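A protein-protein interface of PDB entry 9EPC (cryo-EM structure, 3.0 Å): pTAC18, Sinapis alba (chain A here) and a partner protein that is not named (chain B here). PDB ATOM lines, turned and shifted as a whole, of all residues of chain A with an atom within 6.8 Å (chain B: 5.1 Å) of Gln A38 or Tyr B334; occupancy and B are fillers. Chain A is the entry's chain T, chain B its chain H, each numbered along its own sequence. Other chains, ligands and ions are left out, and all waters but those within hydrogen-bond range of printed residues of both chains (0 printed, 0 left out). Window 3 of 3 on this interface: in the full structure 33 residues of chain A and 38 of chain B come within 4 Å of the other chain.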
ATOM      1  N   MET A  37      28.885  10.642  -2.067  1.00  0.00           N
ATOM      2  CA  MET A  37      28.154  10.781  -3.321  1.00  0.00           C
ATOM      3  C   MET A  37      27.217   9.597  -3.543  1.00  0.00           C
ATOM      4  O   MET A  37      27.526   8.472  -3.155  1.00  0.00           O
ATOM      5  CB  MET A  37      29.131  10.917  -4.494  1.00  0.00           C
ATOM      6  CG  MET A  37      28.483  10.869  -5.872  1.00  0.00           C
ATOM      7  SD  MET A  37      27.140  12.056  -6.071  1.00  0.00           S
ATOM      8  CE  MET A  37      26.439  11.514  -7.629  1.00  0.00           C
ATOM      9  N   GLN A  38      26.069   9.864  -4.160  1.00  0.00           N
ATOM     10  CA  GLN A  38      25.119   8.805  -4.465  1.00  0.00           C
ATOM     11  C   GLN A  38      25.731   7.813  -5.447  1.00  0.00           C
ATOM     12  O   GLN A  38      26.496   8.187  -6.339  1.00  0.00           O
ATOM     13  CB  GLN A  38      23.839   9.396  -5.055  1.00  0.00           C
ATOM     14  CG  GLN A  38      23.381  10.696  -4.410  1.00  0.00           C
ATOM     15  CD  GLN A  38      22.383  10.489  -3.288  1.00  0.00           C
ATOM     16  OE1 GLN A  38      21.674   9.485  -3.246  1.00  0.00           O
ATOM     17  NE2 GLN A  38      22.321  11.446  -2.369  1.00  0.00           N
ATOM     18  N   THR A  39      25.387   6.539  -5.276  1.00  0.00           N
ATOM     19  CA  THR A  39      25.879   5.510  -6.173  1.00  0.00           C
ATOM     20  C   THR A  39      25.272   5.687  -7.565  1.00  0.00           C
ATOM     21  O   THR A  39      24.161   6.205  -7.705  1.00  0.00           O
ATOM     22  CB  THR A  39      25.544   4.121  -5.636  1.00  0.00           C
ATOM     23  OG1 THR A  39      24.123   3.979  -5.530  1.00  0.00           O
ATOM     24  CG2 THR A  39      26.171   3.916  -4.265  1.00  0.00           C
ATOM     25  N   PRO A  40      25.997   5.300  -8.613  1.00  0.00           N
ATOM     26  CA  PRO A  40      25.418   5.332  -9.960  1.00  0.00           C
ATOM     27  C   PRO A  40      24.286   4.325 -10.106  1.00  0.00           C
ATOM     28  O   PRO A  40      24.291   3.258  -9.489  1.00  0.00           O
ATOM     29  CB  PRO A  40      26.603   4.975 -10.863  1.00  0.00           C
ATOM     30  CG  PRO A  40      27.807   5.355 -10.066  1.00  0.00           C
ATOM     31  CD  PRO A  40      27.449   5.060  -8.642  1.00  0.00           C
ATOM     32  N   LEU A  41      23.316   4.671 -10.953  1.00  0.00           N
ATOM     33  CA  LEU A  41      22.142   3.823 -11.129  1.00  0.00           C
ATOM     34  C   LEU A  41      22.483   2.474 -11.740  1.00  0.00           C
ATOM     35  O   LEU A  41      21.673   1.544 -11.655  1.00  0.00           O
ATOM     36  CB  LEU A  41      21.104   4.524 -12.003  1.00  0.00           C
ATOM     37  CG  LEU A  41      20.600   5.900 -11.569  1.00  0.00           C
ATOM     38  CD1 LEU A  41      19.517   6.383 -12.515  1.00  0.00           C
ATOM     39  CD2 LEU A  41      20.090   5.869 -10.139  1.00  0.00           C
ATOM     40  N   GLU A  43      24.962  -0.055 -11.132  1.00  0.00           N
ATOM     41  CA  GLU A  43      25.021  -1.121 -10.144  1.00  0.00           C
ATOM     42  C   GLU A  43      23.943  -0.982  -9.078  1.00  0.00           C
ATOM     43  O   GLU A  43      23.640  -1.965  -8.394  1.00  0.00           O
ATOM     44  CB  GLU A  43      26.405  -1.161  -9.486  1.00  0.00           C
ATOM     45  CG  GLU A  43      26.608  -0.165  -8.361  1.00  0.00           C
ATOM     46  CD  GLU A  43      26.625   1.274  -8.830  1.00  0.00           C
ATOM     47  OE1 GLU A  43      26.789   1.515 -10.044  1.00  0.00           O
ATOM     48  OE2 GLU A  43      26.474   2.168  -7.974  1.00  0.00           O
ATOM     49  N   ARG A 102      17.102  10.687 -12.561  1.00  0.00           N
ATOM     50  CA  ARG A 102      18.418  10.462 -13.135  1.00  0.00           C
ATOM     51  C   ARG A 102      18.307   9.444 -14.262  1.00  0.00           C
ATOM     52  O   ARG A 102      17.556   8.471 -14.167  1.00  0.00           O
ATOM     53  CB  ARG A 102      19.405   9.959 -12.078  1.00  0.00           C
ATOM     54  CG  ARG A 102      19.610  10.900 -10.908  1.00  0.00           C
ATOM     55  CD  ARG A 102      20.234  10.166  -9.732  1.00  0.00           C
ATOM     56  NE  ARG A 102      21.497   9.530 -10.085  1.00  0.00           N
ATOM     57  CZ  ARG A 102      22.177   8.723  -9.282  1.00  0.00           C
ATOM     58  NH1 ARG A 102      21.737   8.420  -8.073  1.00  0.00           N
ATOM     59  NH2 ARG A 102      23.326   8.205  -9.705  1.00  0.00           N
ATOM     60  N   TYR B 247      29.117  17.369   3.426  1.00  0.00           N
ATOM     61  CA  TYR B 247      27.914  16.572   3.634  1.00  0.00           C
ATOM     62  C   TYR B 247      27.407  16.585   5.065  1.00  0.00           C
ATOM     63  O   TYR B 247      26.200  16.701   5.281  1.00  0.00           O
ATOM     64  CB  TYR B 247      28.168  15.126   3.200  1.00  0.00           C
ATOM     65  CG  TYR B 247      28.527  14.999   1.740  1.00  0.00           C
ATOM     66  CD1 TYR B 247      27.983  15.858   0.797  1.00  0.00           C
ATOM     67  CD2 TYR B 247      29.417  14.028   1.306  1.00  0.00           C
ATOM     68  CE1 TYR B 247      28.309  15.749  -0.538  1.00  0.00           C
ATOM     69  CE2 TYR B 247      29.750  13.913  -0.028  1.00  0.00           C
ATOM     70  CZ  TYR B 247      29.192  14.776  -0.946  1.00  0.00           C
ATOM     71  OH  TYR B 247      29.520  14.667  -2.277  1.00  0.00           O
ATOM     72  N   ARG B 255      30.567   9.839  12.759  1.00  0.00           N
ATOM     73  CA  ARG B 255      30.995  10.610  11.605  1.00  0.00           C
ATOM     74  C   ARG B 255      32.510  10.781  11.623  1.00  0.00           C
ATOM     75  O   ARG B 255      33.181  10.513  12.621  1.00  0.00           O
ATOM     76  CB  ARG B 255      30.305  11.974  11.570  1.00  0.00           C
ATOM     77  CG  ARG B 255      28.790  11.920  11.654  1.00  0.00           C
ATOM     78  CD  ARG B 255      28.214  10.828  10.773  1.00  0.00           C
ATOM     79  NE  ARG B 255      28.541  11.014   9.367  1.00  0.00           N
ATOM     80  CZ  ARG B 255      28.355  10.095   8.433  1.00  0.00           C
ATOM     81  NH1 ARG B 255      27.859   8.905   8.725  1.00  0.00           N
ATOM     82  NH2 ARG B 255      28.676  10.374   7.174  1.00  0.00           N
ATOM     83  N   ASP B 332      28.878   2.234   4.112  1.00  0.00           N
ATOM     84  CA  ASP B 332      29.235   3.516   3.519  1.00  0.00           C
ATOM     85  C   ASP B 332      28.896   4.641   4.488  1.00  0.00           C
ATOM     86  O   ASP B 332      27.725   4.789   4.860  1.00  0.00           O
ATOM     87  CB  ASP B 332      28.488   3.700   2.202  1.00  0.00           C
ATOM     88  CG  ASP B 332      28.852   4.987   1.492  1.00  0.00           C
ATOM     89  OD1 ASP B 332      29.919   5.561   1.790  1.00  0.00           O
ATOM     90  OD2 ASP B 332      28.065   5.431   0.629  1.00  0.00           O
ATOM     91  N   PRO B 333      29.866   5.446   4.923  1.00  0.00           N
ATOM     92  CA  PRO B 333      29.541   6.543   5.846  1.00  0.00           C
ATOM     93  C   PRO B 333      28.603   7.573   5.252  1.00  0.00           C
ATOM     94  O   PRO B 333      27.855   8.217   5.996  1.00  0.00           O
ATOM     95  CB  PRO B 333      30.914   7.148   6.164  1.00  0.00           C
ATOM     96  CG  PRO B 333      31.756   6.791   4.993  1.00  0.00           C
ATOM     97  CD  PRO B 333      31.295   5.427   4.574  1.00  0.00           C
ATOM     98  N   TYR B 334      28.628   7.758   3.931  1.00  0.00           N
ATOM     99  CA  TYR B 334      27.756   8.747   3.307  1.00  0.00           C
ATOM    100  C   TYR B 334      26.288   8.381   3.474  1.00  0.00           C
ATOM    101  O   TYR B 334      25.456   9.248   3.765  1.00  0.00           O
ATOM    102  CB  TYR B 334      28.101   8.893   1.827  1.00  0.00           C
ATOM    103  CG  TYR B 334      27.185   9.833   1.083  1.00  0.00           C
ATOM    104  CD1 TYR B 334      27.377  11.205   1.138  1.00  0.00           C
ATOM    105  CD2 TYR B 334      26.128   9.351   0.325  1.00  0.00           C
ATOM    106  CE1 TYR B 334      26.543  12.069   0.462  1.00  0.00           C
ATOM    107  CE2 TYR B 334      25.289  10.207  -0.355  1.00  0.00           C
ATOM    108  CZ  TYR B 334      25.502  11.566  -0.284  1.00  0.00           C
ATOM    109  OH  TYR B 334      24.669  12.425  -0.960  1.00  0.00           O
ATOM    110  N   ARG B 335      25.950   7.106   3.292  1.00  0.00           N
ATOM    111  CA  ARG B 335      24.564   6.662   3.397  1.00  0.00           C
ATOM    112  C   ARG B 335      24.213   6.269   4.829  1.00  0.00           C
ATOM    113  O   ARG B 335      23.290   6.833   5.425  1.00  0.00           O
ATOM    114  CB  ARG B 335      24.317   5.494   2.437  1.00  0.00           C
ATOM    115  CG  ARG B 335      22.940   4.869   2.561  1.00  0.00           C
ATOM    116  CD  ARG B 335      21.845   5.898   2.363  1.00  0.00           C
ATOM    117  NE  ARG B 335      21.983   6.605   1.098  1.00  0.00           N
ATOM    118  CZ  ARG B 335      21.171   7.567   0.686  1.00  0.00           C
ATOM    119  NH1 ARG B 335      20.140   7.960   1.416  1.00  0.00           N
ATOM    120  NH2 ARG B 335      21.397   8.151  -0.486  1.00  0.00           N
ATOM    121  N   PHE B 336      24.939   5.308   5.389  1.00  0.00           N
ATOM    122  CA  PHE B 336      24.678   4.856   6.747  1.00  0.00           C
ATOM    123  C   PHE B 336      25.360   5.785   7.740  1.00  0.00           C
ATOM    124  O   PHE B 336      26.535   6.125   7.576  1.00  0.00           O
ATOM    125  CB  PHE B 336      25.166   3.423   6.932  1.00  0.00           C
ATOM    126  CG  PHE B 336      24.517   2.441   6.004  1.00  0.00           C
ATOM    127  CD1 PHE B 336      25.047   2.196   4.751  1.00  0.00           C
ATOM    128  CD2 PHE B 336      23.371   1.767   6.383  1.00  0.00           C
ATOM    129  CE1 PHE B 336      24.452   1.296   3.898  1.00  0.00           C
ATOM    130  CE2 PHE B 336      22.771   0.867   5.533  1.00  0.00           C
ATOM    131  CZ  PHE B 336      23.312   0.630   4.289  1.00  0.00           C
ATOM    132  N   PHE B 363      21.093   7.942   6.441  1.00  0.00           N
ATOM    133  CA  PHE B 363      20.835   9.346   6.184  1.00  0.00           C
ATOM    134  C   PHE B 363      19.765   9.507   5.111  1.00  0.00           C
ATOM    135  O   PHE B 363      19.369   8.557   4.433  1.00  0.00           O
ATOM    136  CB  PHE B 363      22.111  10.057   5.740  1.00  0.00           C
ATOM    137  CG  PHE B 363      22.994  10.480   6.868  1.00  0.00           C
ATOM    138  CD1 PHE B 363      22.657  11.564   7.653  1.00  0.00           C
ATOM    139  CD2 PHE B 363      24.172   9.813   7.128  1.00  0.00           C
ATOM    140  CE1 PHE B 363      23.471  11.964   8.685  1.00  0.00           C
ATOM    141  CE2 PHE B 363      24.991  10.214   8.156  1.00  0.00           C
ATOM    142  CZ  PHE B 363      24.639  11.288   8.938  1.00  0.00           C
ATOM    143  N   ARG B 365      20.018  12.305   2.383  1.00  0.00           N
ATOM    144  CA  ARG B 365      20.838  13.420   1.942  1.00  0.00           C
ATOM    145  C   ARG B 365      20.020  14.385   1.087  1.00  0.00           C
ATOM    146  O   ARG B 365      18.805  14.247   0.923  1.00  0.00           O
ATOM    147  CB  ARG B 365      22.052  12.903   1.177  1.00  0.00           C
ATOM    148  CG  ARG B 365      22.970  12.032   2.006  1.00  0.00           C
ATOM    149  CD  ARG B 365      23.638  12.836   3.100  1.00  0.00           C
ATOM    150  NE  ARG B 365      24.599  12.038   3.848  1.00  0.00           N
ATOM    151  CZ  ARG B 365      25.409  12.521   4.779  1.00  0.00           C
ATOM    152  NH1 ARG B 365      25.406  13.804   5.097  1.00  0.00           N
ATOM    153  NH2 ARG B 365      26.242  11.697   5.405  1.00  0.00           N
ATOM    154  N   GLY B 367      20.086  15.078  -2.265  1.00  0.00           N
ATOM    155  CA  GLY B 367      19.470  14.439  -3.408  1.00  0.00           C
ATOM    156  C   GLY B 367      19.045  13.015  -3.121  1.00  0.00           C
ATOM    157  O   GLY B 367      19.812  12.071  -3.325  1.00  0.00           O
ATOM    158  N   ASP B 368      17.810  12.854  -2.655  1.00  0.00           N
ATOM    159  CA  ASP B 368      17.208  11.550  -2.404  1.00  0.00           C
ATOM    160  C   ASP B 368      15.764  11.551  -2.873  1.00  0.00           C
ATOM    161  O   ASP B 368      14.863  11.072  -2.178  1.00  0.00           O
ATOM    162  CB  ASP B 368      17.306  11.169  -0.928  1.00  0.00           C
ATOM    163  CG  ASP B 368      18.691  10.692  -0.542  1.00  0.00           C
ATOM    164  OD1 ASP B 368      19.331  10.001  -1.362  1.00  0.00           O
ATOM    165  OD2 ASP B 368      19.141  11.006   0.578  1.00  0.00           O
ATOM    166  N   ASP B 377      19.852   1.677  -2.288  1.00  0.00           N
ATOM    167  CA  ASP B 377      21.213   1.946  -1.837  1.00  0.00           C
ATOM    168  C   ASP B 377      21.537   1.153  -0.579  1.00  0.00           C
ATOM    169  O   ASP B 377      22.627   0.583  -0.456  1.00  0.00           O
ATOM    170  CB  ASP B 377      21.397   3.443  -1.596  1.00  0.00           C
ATOM    171  CG  ASP B 377      22.854   3.847  -1.515  1.00  0.00           C
ATOM    172  OD1 ASP B 377      23.725   2.969  -1.681  1.00  0.00           O
ATOM    173  OD2 ASP B 377      23.127   5.044  -1.291  1.00  0.00           O
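The side-chain hydroxyl (OH) of Tyr B334 sits at hydrogen-bond distance from the side-chain amide nitrogen (NE2) of Gln A38 (2.9 Å). The guanidinium group (NH2) of Arg B335 sits at hydrogen-bond distance from the side-chain amide oxygen (OE1) of Gln A38 (3.1 Å). O of Gly B367 lies within hydrogen-bond range of NE2 of Gln A38 (2.8 Å). The side-chain carboxylate (OD1) of Asp B368 sits close to the side-chain amide oxygen (OE1) of Gln A38 (3.1 Å).
NH2 of Arg A102 is in hydrogen-bond range of O of Thr A39, 2.9 Å away. The backbone carbonyl oxygen (O) of Tyr B247 sits at hydrogen-bond distance from the guanidinium group (NH1) of Arg B365, at 3.0 Å. OD1 of Asp B332 sits close to N of Tyr B334, 3.3 Å away. O of Arg B335 lies within hydrogen-bond range of N of Phe B363. The guanidinium group (NH2) of Arg B335 lies within salt-bridge range of the side-chain carboxylate (OD1) of Asp B368 (2.9 Å). The side-chain carboxylate (OD2) of Asp B377 is in salt-bridge range of the guanidinium group (NE) of Arg B335 (3.1 Å).
Met A37 touches Tyr B247. Tyr B334 touches Met A37 (CD1 to N, 3.6 Å). CB of Arg B365 touches NE2 of Gln A38 (3.8 Å). Asp B377 touches Thr A39 (OD1 to CG2, 3.7 Å).
Gln A38 touches five residues of chain B. Of chain A, only Met A37 and Gln A38 come within 4 Å of Tyr B334. Printed residues of chain A within 4 Å of Arg B365: Gln A38 (3.8 Å). Of the printed residues of chain B, Thr A39 touches Asp B377. Of the printed residues of chain A, Asp B377 touches Thr A39.
Along chain A the printed residues that touch a printed residue of chain B span positions 37 to 39. Of the 12 printed residues of chain B, 7 touch a printed residue of chain A. Hydrophobic or aromatic side chains of chain B that line the printed part of chain A: Tyr B247 and Tyr B334. Among the printed residues, 8 pairs touch across the chains.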
